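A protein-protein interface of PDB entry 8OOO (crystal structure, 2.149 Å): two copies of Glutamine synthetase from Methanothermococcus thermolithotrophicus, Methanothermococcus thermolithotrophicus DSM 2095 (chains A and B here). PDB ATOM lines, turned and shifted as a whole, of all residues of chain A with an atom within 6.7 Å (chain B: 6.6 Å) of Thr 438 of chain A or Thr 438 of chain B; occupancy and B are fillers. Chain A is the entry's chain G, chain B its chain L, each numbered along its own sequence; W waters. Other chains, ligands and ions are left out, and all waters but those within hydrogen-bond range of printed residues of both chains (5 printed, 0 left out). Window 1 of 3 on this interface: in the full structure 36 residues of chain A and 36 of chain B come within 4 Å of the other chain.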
ATOM      1  N   MET A 237       9.080 -23.028   0.056  1.00  0.00           N
ATOM      2  CA  MET A 237      10.161 -22.068  -0.119  1.00  0.00           C
ATOM      3  C   MET A 237       9.629 -20.853  -0.890  1.00  0.00           C
ATOM      4  O   MET A 237       8.990 -21.040  -1.935  1.00  0.00           O
ATOM      5  CB  MET A 237      11.291 -22.715  -0.929  1.00  0.00           C
ATOM      6  CG  MET A 237      12.521 -21.818  -1.103  1.00  0.00           C
ATOM      7  SD  MET A 237      13.892 -22.777  -1.756  1.00  0.00           S
ATOM      8  CE  MET A 237      15.096 -21.482  -2.036  1.00  0.00           C
ATOM      9  N   VAL A 298      16.016 -15.564   4.359  1.00  0.00           N
ATOM     10  CA  VAL A 298      16.819 -14.824   3.376  1.00  0.00           C
ATOM     11  C   VAL A 298      16.101 -14.870   2.013  1.00  0.00           C
ATOM     12  O   VAL A 298      16.011 -13.854   1.301  1.00  0.00           O
ATOM     13  CB  VAL A 298      18.233 -15.432   3.264  1.00  0.00           C
ATOM     14  CG1 VAL A 298      18.979 -14.905   2.023  1.00  0.00           C
ATOM     15  CG2 VAL A 298      19.008 -15.188   4.553  1.00  0.00           C
ATOM     16  N   ASN A 299      15.618 -16.054   1.656  1.00  0.00           N
ATOM     17  CA  ASN A 299      14.999 -16.300   0.367  1.00  0.00           C
ATOM     18  C   ASN A 299      13.703 -15.518   0.178  1.00  0.00           C
ATOM     19  O   ASN A 299      13.327 -15.230  -0.951  1.00  0.00           O
ATOM     20  CB  ASN A 299      14.791 -17.797   0.193  1.00  0.00           C
ATOM     21  CG  ASN A 299      14.182 -18.171  -1.124  1.00  0.00           C
ATOM     22  OD1 ASN A 299      13.045 -18.667  -1.169  1.00  0.00           O
ATOM     23  ND2 ASN A 299      14.902 -17.926  -2.209  1.00  0.00           N
ATOM     24  N   LYS A 302      13.904 -12.633  -2.191  1.00  0.00           N
ATOM     25  CA  LYS A 302      14.144 -12.897  -3.614  1.00  0.00           C
ATOM     26  C   LYS A 302      12.767 -12.888  -4.331  1.00  0.00           C
ATOM     27  O   LYS A 302      12.699 -12.746  -5.556  1.00  0.00           O
ATOM     28  CB  LYS A 302      14.941 -14.208  -3.833  1.00  0.00           C
ATOM     29  CG  LYS A 302      16.457 -14.039  -3.709  1.00  0.00           C
ATOM     30  CD  LYS A 302      16.937 -13.684  -2.321  1.00  0.00           C
ATOM     31  CE  LYS A 302      18.353 -13.146  -2.312  1.00  0.00           C
ATOM     32  NZ  LYS A 302      19.352 -14.072  -2.929  1.00  0.00           N
ATOM     33  N   PHE A 433      24.382 -16.926   5.956  1.00  0.00           N
ATOM     34  CA  PHE A 433      24.216 -16.585   4.564  1.00  0.00           C
ATOM     35  C   PHE A 433      25.292 -15.586   4.101  1.00  0.00           C
ATOM     36  O   PHE A 433      25.921 -15.792   3.047  1.00  0.00           O
ATOM     37  CB  PHE A 433      22.798 -16.035   4.314  1.00  0.00           C
ATOM     38  CG  PHE A 433      22.605 -15.447   2.923  1.00  0.00           C
ATOM     39  CD1 PHE A 433      22.690 -16.250   1.794  1.00  0.00           C
ATOM     40  CD2 PHE A 433      22.326 -14.101   2.758  1.00  0.00           C
ATOM     41  CE1 PHE A 433      22.464 -15.714   0.523  1.00  0.00           C
ATOM     42  CE2 PHE A 433      22.153 -13.562   1.477  1.00  0.00           C
ATOM     43  CZ  PHE A 433      22.243 -14.360   0.366  1.00  0.00           C
ATOM     44  N   SER A 436      28.825 -17.101   3.554  1.00  0.00           N
ATOM     45  CA  SER A 436      28.973 -18.175   2.582  1.00  0.00           C
ATOM     46  C   SER A 436      29.452 -17.649   1.255  1.00  0.00           C
ATOM     47  O   SER A 436      29.210 -16.495   0.935  1.00  0.00           O
ATOM     48  CB  SER A 436      27.636 -18.888   2.395  1.00  0.00           C
ATOM     49  OG  SER A 436      26.775 -18.093   1.588  1.00  0.00           O
ATOM     50  N   VAL A 437      30.072 -18.511   0.453  1.00  0.00           N
ATOM     51  CA  VAL A 437      30.459 -18.160  -0.914  1.00  0.00           C
ATOM     52  C   VAL A 437      29.409 -18.821  -1.830  1.00  0.00           C
ATOM     53  O   VAL A 437      29.331 -20.060  -1.911  1.00  0.00           O
ATOM     54  CB  VAL A 437      31.885 -18.633  -1.249  1.00  0.00           C
ATOM     55  CG1 VAL A 437      32.232 -18.310  -2.705  1.00  0.00           C
ATOM     56  CG2 VAL A 437      32.904 -18.030  -0.275  1.00  0.00           C
ATOM     57  N   THR A 438      28.567 -18.004  -2.458  1.00  0.00           N
ATOM     58  CA  THR A 438      27.490 -18.515  -3.290  1.00  0.00           C
ATOM     59  C   THR A 438      27.920 -18.895  -4.713  1.00  0.00           C
ATOM     60  O   THR A 438      28.998 -18.529  -5.186  1.00  0.00           O
ATOM     61  CB  THR A 438      26.359 -17.501  -3.315  1.00  0.00           C
ATOM     62  OG1 THR A 438      26.776 -16.334  -4.024  1.00  0.00           O
ATOM     63  CG2 THR A 438      25.878 -17.147  -1.932  1.00  0.00           C
ATOM     64  N   ASP A 439      27.069 -19.673  -5.386  1.00  0.00           N
ATOM     65  CA  ASP A 439      27.316 -20.063  -6.773  1.00  0.00           C
ATOM     66  C   ASP A 439      27.299 -18.838  -7.686  1.00  0.00           C
ATOM     67  O   ASP A 439      28.070 -18.804  -8.661  1.00  0.00           O
ATOM     68  CB  ASP A 439      26.314 -21.127  -7.245  1.00  0.00           C
ATOM     69  CG  ASP A 439      24.842 -20.805  -7.020  1.00  0.00           C
ATOM     70  OD1 ASP A 439      24.536 -19.746  -6.363  1.00  0.00           O
ATOM     71  OD2 ASP A 439      23.993 -21.602  -7.471  1.00  0.00           O
ATOM     72  N   TRP A 440      26.471 -17.818  -7.377  1.00  0.00           N
ATOM     73  CA  TRP A 440      26.409 -16.593  -8.198  1.00  0.00           C
ATOM     74  C   TRP A 440      27.794 -15.943  -8.265  1.00  0.00           C
ATOM     75  O   TRP A 440      28.277 -15.591  -9.369  1.00  0.00           O
ATOM     76  CB  TRP A 440      25.371 -15.591  -7.638  1.00  0.00           C
ATOM     77  CG  TRP A 440      25.217 -14.340  -8.476  1.00  0.00           C
ATOM     78  CD1 TRP A 440      24.295 -14.122  -9.459  1.00  0.00           C
ATOM     79  CD2 TRP A 440      26.012 -13.131  -8.398  1.00  0.00           C
ATOM     80  NE1 TRP A 440      24.436 -12.834  -9.968  1.00  0.00           N
ATOM     81  CE2 TRP A 440      25.545 -12.254  -9.408  1.00  0.00           C
ATOM     82  CE3 TRP A 440      27.142 -12.756  -7.663  1.00  0.00           C
ATOM     83  CZ2 TRP A 440      26.117 -11.007  -9.636  1.00  0.00           C
ATOM     84  CZ3 TRP A 440      27.697 -11.509  -7.883  1.00  0.00           C
ATOM     85  CH2 TRP A 440      27.200 -10.659  -8.870  1.00  0.00           C
ATOM     86  N   GLU A 441      28.455 -15.865  -7.099  1.00  0.00           N
ATOM     87  CA  GLU A 441      29.791 -15.293  -6.958  1.00  0.00           C
ATOM     88  C   GLU A 441      30.846 -16.089  -7.705  1.00  0.00           C
ATOM     89  O   GLU A 441      31.730 -15.500  -8.300  1.00  0.00           O
ATOM     90  CB  GLU A 441      30.173 -15.198  -5.463  1.00  0.00           C
ATOM     91  CG  GLU A 441      29.314 -14.233  -4.669  1.00  0.00           C
ATOM     92  CD  GLU A 441      29.479 -14.436  -3.171  1.00  0.00           C
ATOM     93  OE1 GLU A 441      28.568 -15.021  -2.540  1.00  0.00           O
ATOM     94  OE2 GLU A 441      30.541 -14.048  -2.631  1.00  0.00           O
ATOM     95  N   THR A 442      30.801 -17.423  -7.632  1.00  0.00           N
ATOM     96  CA  THR A 442      31.766 -18.266  -8.348  1.00  0.00           C
ATOM     97  C   THR A 442      31.618 -18.035  -9.852  1.00  0.00           C
ATOM     98  O   THR A 442      32.611 -17.892 -10.564  1.00  0.00           O
ATOM     99  CB  THR A 442      31.560 -19.758  -7.970  1.00  0.00           C
ATOM    100  OG1 THR A 442      31.897 -19.935  -6.582  1.00  0.00           O
ATOM    101  CG2 THR A 442      32.385 -20.724  -8.856  1.00  0.00           C
ATOM    102  N   THR A 443      30.372 -17.972 -10.337  1.00  0.00           N
ATOM    103  CA  THR A 443      30.130 -17.723 -11.757  1.00  0.00           C
ATOM    104  C   THR A 443      30.625 -16.330 -12.149  1.00  0.00           C
ATOM    105  O   THR A 443      31.237 -16.162 -13.205  1.00  0.00           O
ATOM    106  CB  THR A 443      28.623 -17.876 -12.058  1.00  0.00           C
ATOM    107  OG1 THR A 443      28.277 -19.256 -11.830  1.00  0.00           O
ATOM    108  CG2 THR A 443      28.261 -17.463 -13.476  1.00  0.00           C
ATOM    109  N   MET B 237      39.989 -13.830  -7.405  1.00  0.00           N
ATOM    110  CA  MET B 237      38.716 -13.731  -6.678  1.00  0.00           C
ATOM    111  C   MET B 237      39.009 -13.543  -5.174  1.00  0.00           C
ATOM    112  O   MET B 237      39.822 -14.304  -4.630  1.00  0.00           O
ATOM    113  CB  MET B 237      37.906 -15.027  -6.877  1.00  0.00           C
ATOM    114  CG  MET B 237      36.541 -14.994  -6.247  1.00  0.00           C
ATOM    115  SD  MET B 237      35.604 -16.393  -6.794  1.00  0.00           S
ATOM    116  CE  MET B 237      34.122 -16.257  -5.763  1.00  0.00           C
ATOM    117  N   VAL B 298      30.813  -8.178  -4.944  1.00  0.00           N
ATOM    118  CA  VAL B 298      29.974  -8.761  -3.907  1.00  0.00           C
ATOM    119  C   VAL B 298      30.854  -9.682  -3.033  1.00  0.00           C
ATOM    120  O   VAL B 298      30.779  -9.650  -1.806  1.00  0.00           O
ATOM    121  CB  VAL B 298      28.805  -9.554  -4.544  1.00  0.00           C
ATOM    122  CG1 VAL B 298      28.119 -10.454  -3.502  1.00  0.00           C
ATOM    123  CG2 VAL B 298      27.811  -8.601  -5.206  1.00  0.00           C
ATOM    124  N   ASN B 299      31.670 -10.503  -3.693  1.00  0.00           N
ATOM    125  CA  ASN B 299      32.508 -11.507  -3.061  1.00  0.00           C
ATOM    126  C   ASN B 299      33.586 -10.895  -2.135  1.00  0.00           C
ATOM    127  O   ASN B 299      34.023 -11.553  -1.193  1.00  0.00           O
ATOM    128  CB  ASN B 299      33.129 -12.397  -4.129  1.00  0.00           C
ATOM    129  CG  ASN B 299      33.959 -13.497  -3.571  1.00  0.00           C
ATOM    130  OD1 ASN B 299      35.169 -13.513  -3.757  1.00  0.00           O
ATOM    131  ND2 ASN B 299      33.339 -14.444  -2.875  1.00  0.00           N
ATOM    132  N   LYS B 302      32.921 -11.221   1.523  1.00  0.00           N
ATOM    133  CA  LYS B 302      32.954 -12.567   2.104  1.00  0.00           C
ATOM    134  C   LYS B 302      34.362 -12.776   2.722  1.00  0.00           C
ATOM    135  O   LYS B 302      34.541 -13.648   3.566  1.00  0.00           O
ATOM    136  CB  LYS B 302      32.572 -13.650   1.078  1.00  0.00           C
ATOM    137  CG  LYS B 302      31.055 -13.869   0.956  1.00  0.00           C
ATOM    138  CD  LYS B 302      30.315 -12.718   0.320  1.00  0.00           C
ATOM    139  CE  LYS B 302      28.817 -12.816   0.525  1.00  0.00           C
ATOM    140  NZ  LYS B 302      28.238 -14.068  -0.011  1.00  0.00           N
ATOM    141  N   PHE B 433      22.990  -9.849  -8.162  1.00  0.00           N
ATOM    142  CA  PHE B 433      23.252 -10.759  -7.053  1.00  0.00           C
ATOM    143  C   PHE B 433      22.030 -10.881  -6.153  1.00  0.00           C
ATOM    144  O   PHE B 433      21.647 -11.986  -5.817  1.00  0.00           O
ATOM    145  CB  PHE B 433      24.486 -10.291  -6.273  1.00  0.00           C
ATOM    146  CG  PHE B 433      24.717 -11.013  -4.969  1.00  0.00           C
ATOM    147  CD1 PHE B 433      24.981 -12.375  -4.948  1.00  0.00           C
ATOM    148  CD2 PHE B 433      24.616 -10.345  -3.754  1.00  0.00           C
ATOM    149  CE1 PHE B 433      25.215 -13.042  -3.737  1.00  0.00           C
ATOM    150  CE2 PHE B 433      24.824 -11.017  -2.548  1.00  0.00           C
ATOM    151  CZ  PHE B 433      25.145 -12.356  -2.550  1.00  0.00           C
ATOM    152  N   SER B 436      19.137 -13.077  -7.514  1.00  0.00           N
ATOM    153  CA  SER B 436      19.414 -14.472  -7.827  1.00  0.00           C
ATOM    154  C   SER B 436      19.003 -15.372  -6.665  1.00  0.00           C
ATOM    155  O   SER B 436      18.982 -14.933  -5.520  1.00  0.00           O
ATOM    156  CB  SER B 436      20.902 -14.662  -8.112  1.00  0.00           C
ATOM    157  OG  SER B 436      21.611 -14.654  -6.887  1.00  0.00           O
ATOM    158  N   VAL B 437      18.753 -16.645  -6.957  1.00  0.00           N
ATOM    159  CA  VAL B 437      18.458 -17.658  -5.938  1.00  0.00           C
ATOM    160  C   VAL B 437      19.742 -18.467  -5.781  1.00  0.00           C
ATOM    161  O   VAL B 437      20.171 -19.164  -6.723  1.00  0.00           O
ATOM    162  CB  VAL B 437      17.269 -18.556  -6.328  1.00  0.00           C
ATOM    163  CG1 VAL B 437      17.016 -19.599  -5.245  1.00  0.00           C
ATOM    164  CG2 VAL B 437      16.011 -17.710  -6.589  1.00  0.00           C
ATOM    165  N   THR B 438      20.417 -18.303  -4.639  1.00  0.00           N
ATOM    166  CA  THR B 438      21.695 -18.975  -4.422  1.00  0.00           C
ATOM    167  C   THR B 438      21.562 -20.429  -3.978  1.00  0.00           C
ATOM    168  O   THR B 438      20.490 -20.875  -3.578  1.00  0.00           O
ATOM    169  CB  THR B 438      22.536 -18.166  -3.464  1.00  0.00           C
ATOM    170  OG1 THR B 438      21.935 -18.204  -2.176  1.00  0.00           O
ATOM    171  CG2 THR B 438      22.723 -16.713  -3.943  1.00  0.00           C
ATOM    172  N   ASP B 439      22.664 -21.185  -4.088  1.00  0.00           N
ATOM    173  CA  ASP B 439      22.712 -22.566  -3.615  1.00  0.00           C
ATOM    174  C   ASP B 439      22.529 -22.611  -2.101  1.00  0.00           C
ATOM    175  O   ASP B 439      21.943 -23.578  -1.603  1.00  0.00           O
ATOM    176  CB  ASP B 439      24.032 -23.255  -4.035  1.00  0.00           C
ATOM    177  CG  ASP B 439      25.321 -22.476  -3.737  1.00  0.00           C
ATOM    178  OD1 ASP B 439      25.230 -21.306  -3.293  1.00  0.00           O
ATOM    179  OD2 ASP B 439      26.413 -23.022  -3.985  1.00  0.00           O
ATOM    180  N   TRP B 440      23.019 -21.596  -1.356  1.00  0.00           N
ATOM    181  CA  TRP B 440      22.895 -21.558   0.108  1.00  0.00           C
ATOM    182  C   TRP B 440      21.414 -21.600   0.484  1.00  0.00           C
ATOM    183  O   TRP B 440      21.012 -22.398   1.351  1.00  0.00           O
ATOM    184  CB  TRP B 440      23.566 -20.303   0.711  1.00  0.00           C
ATOM    185  CG  TRP B 440      23.514 -20.251   2.228  1.00  0.00           C
ATOM    186  CD1 TRP B 440      24.499 -20.616   3.094  1.00  0.00           C
ATOM    187  CD2 TRP B 440      22.415 -19.790   3.047  1.00  0.00           C
ATOM    188  NE1 TRP B 440      24.093 -20.410   4.393  1.00  0.00           N
ATOM    189  CE2 TRP B 440      22.793 -19.968   4.393  1.00  0.00           C
ATOM    190  CE3 TRP B 440      21.140 -19.279   2.772  1.00  0.00           C
ATOM    191  CZ2 TRP B 440      21.965 -19.586   5.460  1.00  0.00           C
ATOM    192  CZ3 TRP B 440      20.307 -18.937   3.826  1.00  0.00           C
ATOM    193  CH2 TRP B 440      20.708 -19.129   5.154  1.00  0.00           C
ATOM    194  N   GLU B 441      20.596 -20.805  -0.246  1.00  0.00           N
ATOM    195  CA  GLU B 441      19.156 -20.720  -0.035  1.00  0.00           C
ATOM    196  C   GLU B 441      18.448 -22.029  -0.379  1.00  0.00           C
ATOM    197  O   GLU B 441      17.526 -22.409   0.307  1.00  0.00           O
ATOM    198  CB  GLU B 441      18.573 -19.576  -0.866  1.00  0.00           C
ATOM    199  CG  GLU B 441      19.045 -18.195  -0.445  1.00  0.00           C
ATOM    200  CD  GLU B 441      18.726 -17.165  -1.518  1.00  0.00           C
ATOM    201  OE1 GLU B 441      19.659 -16.761  -2.256  1.00  0.00           O
ATOM    202  OE2 GLU B 441      17.529 -16.818  -1.668  1.00  0.00           O
ATOM    203  N   THR B 442      18.830 -22.705  -1.461  1.00  0.00           N
ATOM    204  CA  THR B 442      18.220 -23.974  -1.838  1.00  0.00           C
ATOM    205  C   THR B 442      18.491 -24.994  -0.752  1.00  0.00           C
ATOM    206  O   THR B 442      17.590 -25.728  -0.383  1.00  0.00           O
ATOM    207  CB  THR B 442      18.755 -24.438  -3.226  1.00  0.00           C
ATOM    208  OG1 THR B 442      18.278 -23.541  -4.216  1.00  0.00           O
ATOM    209  CG2 THR B 442      18.314 -25.889  -3.590  1.00  0.00           C
ATOM    210  N   THR B 443      19.737 -25.052  -0.252  1.00  0.00           N
ATOM    211  CA  THR B 443      20.096 -25.996   0.801  1.00  0.00           C
ATOM    212  C   THR B 443      19.300 -25.672   2.076  1.00  0.00           C
ATOM    213  O   THR B 443      18.822 -26.586   2.762  1.00  0.00           O
ATOM    214  CB  THR B 443      21.622 -25.905   1.108  1.00  0.00           C
ATOM    215  OG1 THR B 443      22.393 -26.305  -0.014  1.00  0.00           O
ATOM    216  CG2 THR B 443      22.028 -26.730   2.315  1.00  0.00           C
HETATM  217  O   HOH W   1      21.325 -21.483  -7.449  1.00  0.00           O
HETATM  218  O   HOH W   2      22.660 -18.237  -8.189  1.00  0.00           O
HETATM  219  O   HOH W   3      21.749 -12.980  -3.151  1.00  0.00           O
HETATM  220  O   HOH W   4      26.783 -21.374  -0.622  1.00  0.00           O
HETATM  221  O   HOH W   5      25.550 -14.395   0.744  1.00  0.00           O
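The backbone carbonyl oxygen of Ser 436 of chain A is in hydrogen-bond range of the side-chain amino group of Lys 302 of chain B (2.8 Å). The side-chain amino group (NZ) of Lys 302 of chain B lies within salt-bridge range of the side-chain carboxylate (OE1) of Glu 441 of chain A (2.7 Å). The side-chain amide nitrogen of Asn 299 of chain B lies within hydrogen-bond range of the side-chain carboxylate of Glu 441 of chain A (2.8 Å). The backbone NH (N) of Asp 439 of chain A lies within hydrogen-bond range of the side-chain carboxylate (OD1) of Asp 439 of chain B (3.2 Å). The side-chain amide nitrogen (ND2) of Asn 299 of chain A sits at hydrogen-bond distance from the side-chain carboxylate (OE2) of Glu 441 of chain B. NZ of Lys 302 of chain A is in hydrogen-bond range of O of Ser 436 of chain B, 2.8 Å away. The side-chain carboxylate (OE1) of Glu 441 of chain B lies within salt-bridge range of the side-chain amino group (NZ) of Lys 302 of chain A (2.8 Å).
OE1 of Glu 441 of chain B is in hydrogen-bond range of OG1 of Thr 438 of chain B. OE1 of Glu 441 of chain A sits at hydrogen-bond distance from OG1 of Thr 438 of chain A, 2.7 Å away. The side-chain hydroxyl of Ser 436 of chain B lies within hydrogen-bond range of the backbone carbonyl oxygen of Phe 433 of chain B. The backbone carbonyl oxygen of Asp 439 of chain A is in hydrogen-bond range of the side-chain hydroxyl of Thr 443 of chain A (3.2 Å). OG1 of Thr 443 of chain B is in hydrogen-bond range of O of Asp 439 of chain B (3.2 Å). O of Phe 433 of chain A sits at hydrogen-bond distance from OG of Ser 436 of chain A.
Glu 441 of chain B touches Met 237 of chain A. Met 237 of chain A touches Thr 442 of chain B (CE to N, 3.97 Å). Trp 440 of chain B touches Phe 433 of chain A. CD1 of Trp 440 of chain B touches CB of Ser 436 of chain A, at 3.6 Å. Thr 438 of chain A touches Thr 438 of chain B (CG2 to CG2, 3.8 Å). Thr 438 of chain A touches Asp 439 of chain B (CA to OD1, 3.6 Å). Asp 439 of chain A touches Thr 438 of chain B (OD1 to CA, 3.5 Å). Trp 440 of chain A touches Val 298 of chain B (CZ3 to CG2, 3.95 Å). Trp 440 of chain A touches Ser 436 of chain B (CD1 to CB, 3.7 Å). Thr 442 of chain A touches Met 237 of chain B (N to CE, 3.99 Å).
Val 298 of chain A touches none of the printed residues of chain B. Of the printed residues of chain B, Phe 433 of chain A touches Thr 438 (3.7 Å) and Trp 440 (3.5 Å). Thr 438 of chain A touches just these residues of chain B: Phe 433 (3.7 Å), Thr 438 (3.8 Å) and Asp 439 (3.6 Å). Of the printed residues of chain B, Trp 440 of chain A touches Val 298, Phe 433 and Ser 436. Of the printed residues of chain B, Glu 441 of chain A touches Met 237, Asn 299 and Lys 302. Of the printed residues of chain B, Thr 442 of chain A touches Met 237. Thr 443 of chain B touches none of the printed residues of chain A. The nearest residue of chain B that does not touch Thr 438 of chain A is Lys 302 of chain B (4.3 Å). The nearest residue of chain A that does not touch Thr 438 of chain B is Lys 302 of chain A (4.4 Å). The nearest printed residue of chain A that does not touch Phe 433 of chain B is Glu 441 of chain A (4.1 Å).
Of the 13 printed residues of chain A, 10 touch a printed residue of chain B. Printed residues of chain A that touch a printed residue of chain B: Met 237, Asn 299, Lys 302, Phe 433, Ser 436, Thr 438, Asp 439, Trp 440, Glu 441 and Thr 442. Hydrophobic or aromatic side chains of chain A within 4 Å of the printed part of chain B: Met 237, Phe 433 and Trp 440. Of the 13 printed residues of chain B, 11 touch a printed residue of chain A. Among the printed residues, 21 pairs touch across the chains.
Met 237 of chain A touches Thr 442 of chain B, and with the chains exchanged Thr 442 of chain A touches Met 237 of chain B. Asn 299 of chain A touches Glu 441 of chain B, and with the chains exchanged Glu 441 of chain A touches Asn 299 of chain B. Thr 438 of chain A touches its own counterpart, Thr 438 of chain B. Thr 438 of chain A touches Asp 439 of chain B, and with the chains exchanged Asp 439 of chain A touches Thr 438 of chain B. Positions printed for both chains: 237, 298, 299, 302, 433, 436, 437, 438, 439, 440, 441, 442 and 443.
Water W3 lies within hydrogen-bond range of the side-chain amino group of Lys 302 of chain A (2.6 Å) and the backbone carbonyl oxygen of Phe 433 of chain B (2.8 Å). Water W1 bridges the side-chain carboxylate (OD2) of Asp 439 of chain A (2.7 Å) and the backbone carbonyl oxygen (O) of Val 437 of chain B (2.7 Å). Water W5 lies within hydrogen-bond range of the backbone carbonyl oxygen of Phe 433 of chain A (2.7 Å) and the side-chain amino group of Lys 302 of chain B (2.8 Å). Water W2 lies within hydrogen-bond range of OD1 of Asp 439 of chain A and O of Val 437 of chain B. Water W4 lies within hydrogen-bond range of OD1 of Asp 439 of chain B (3.1 Å) and O of Val 437 of chain A (3.1 Å).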
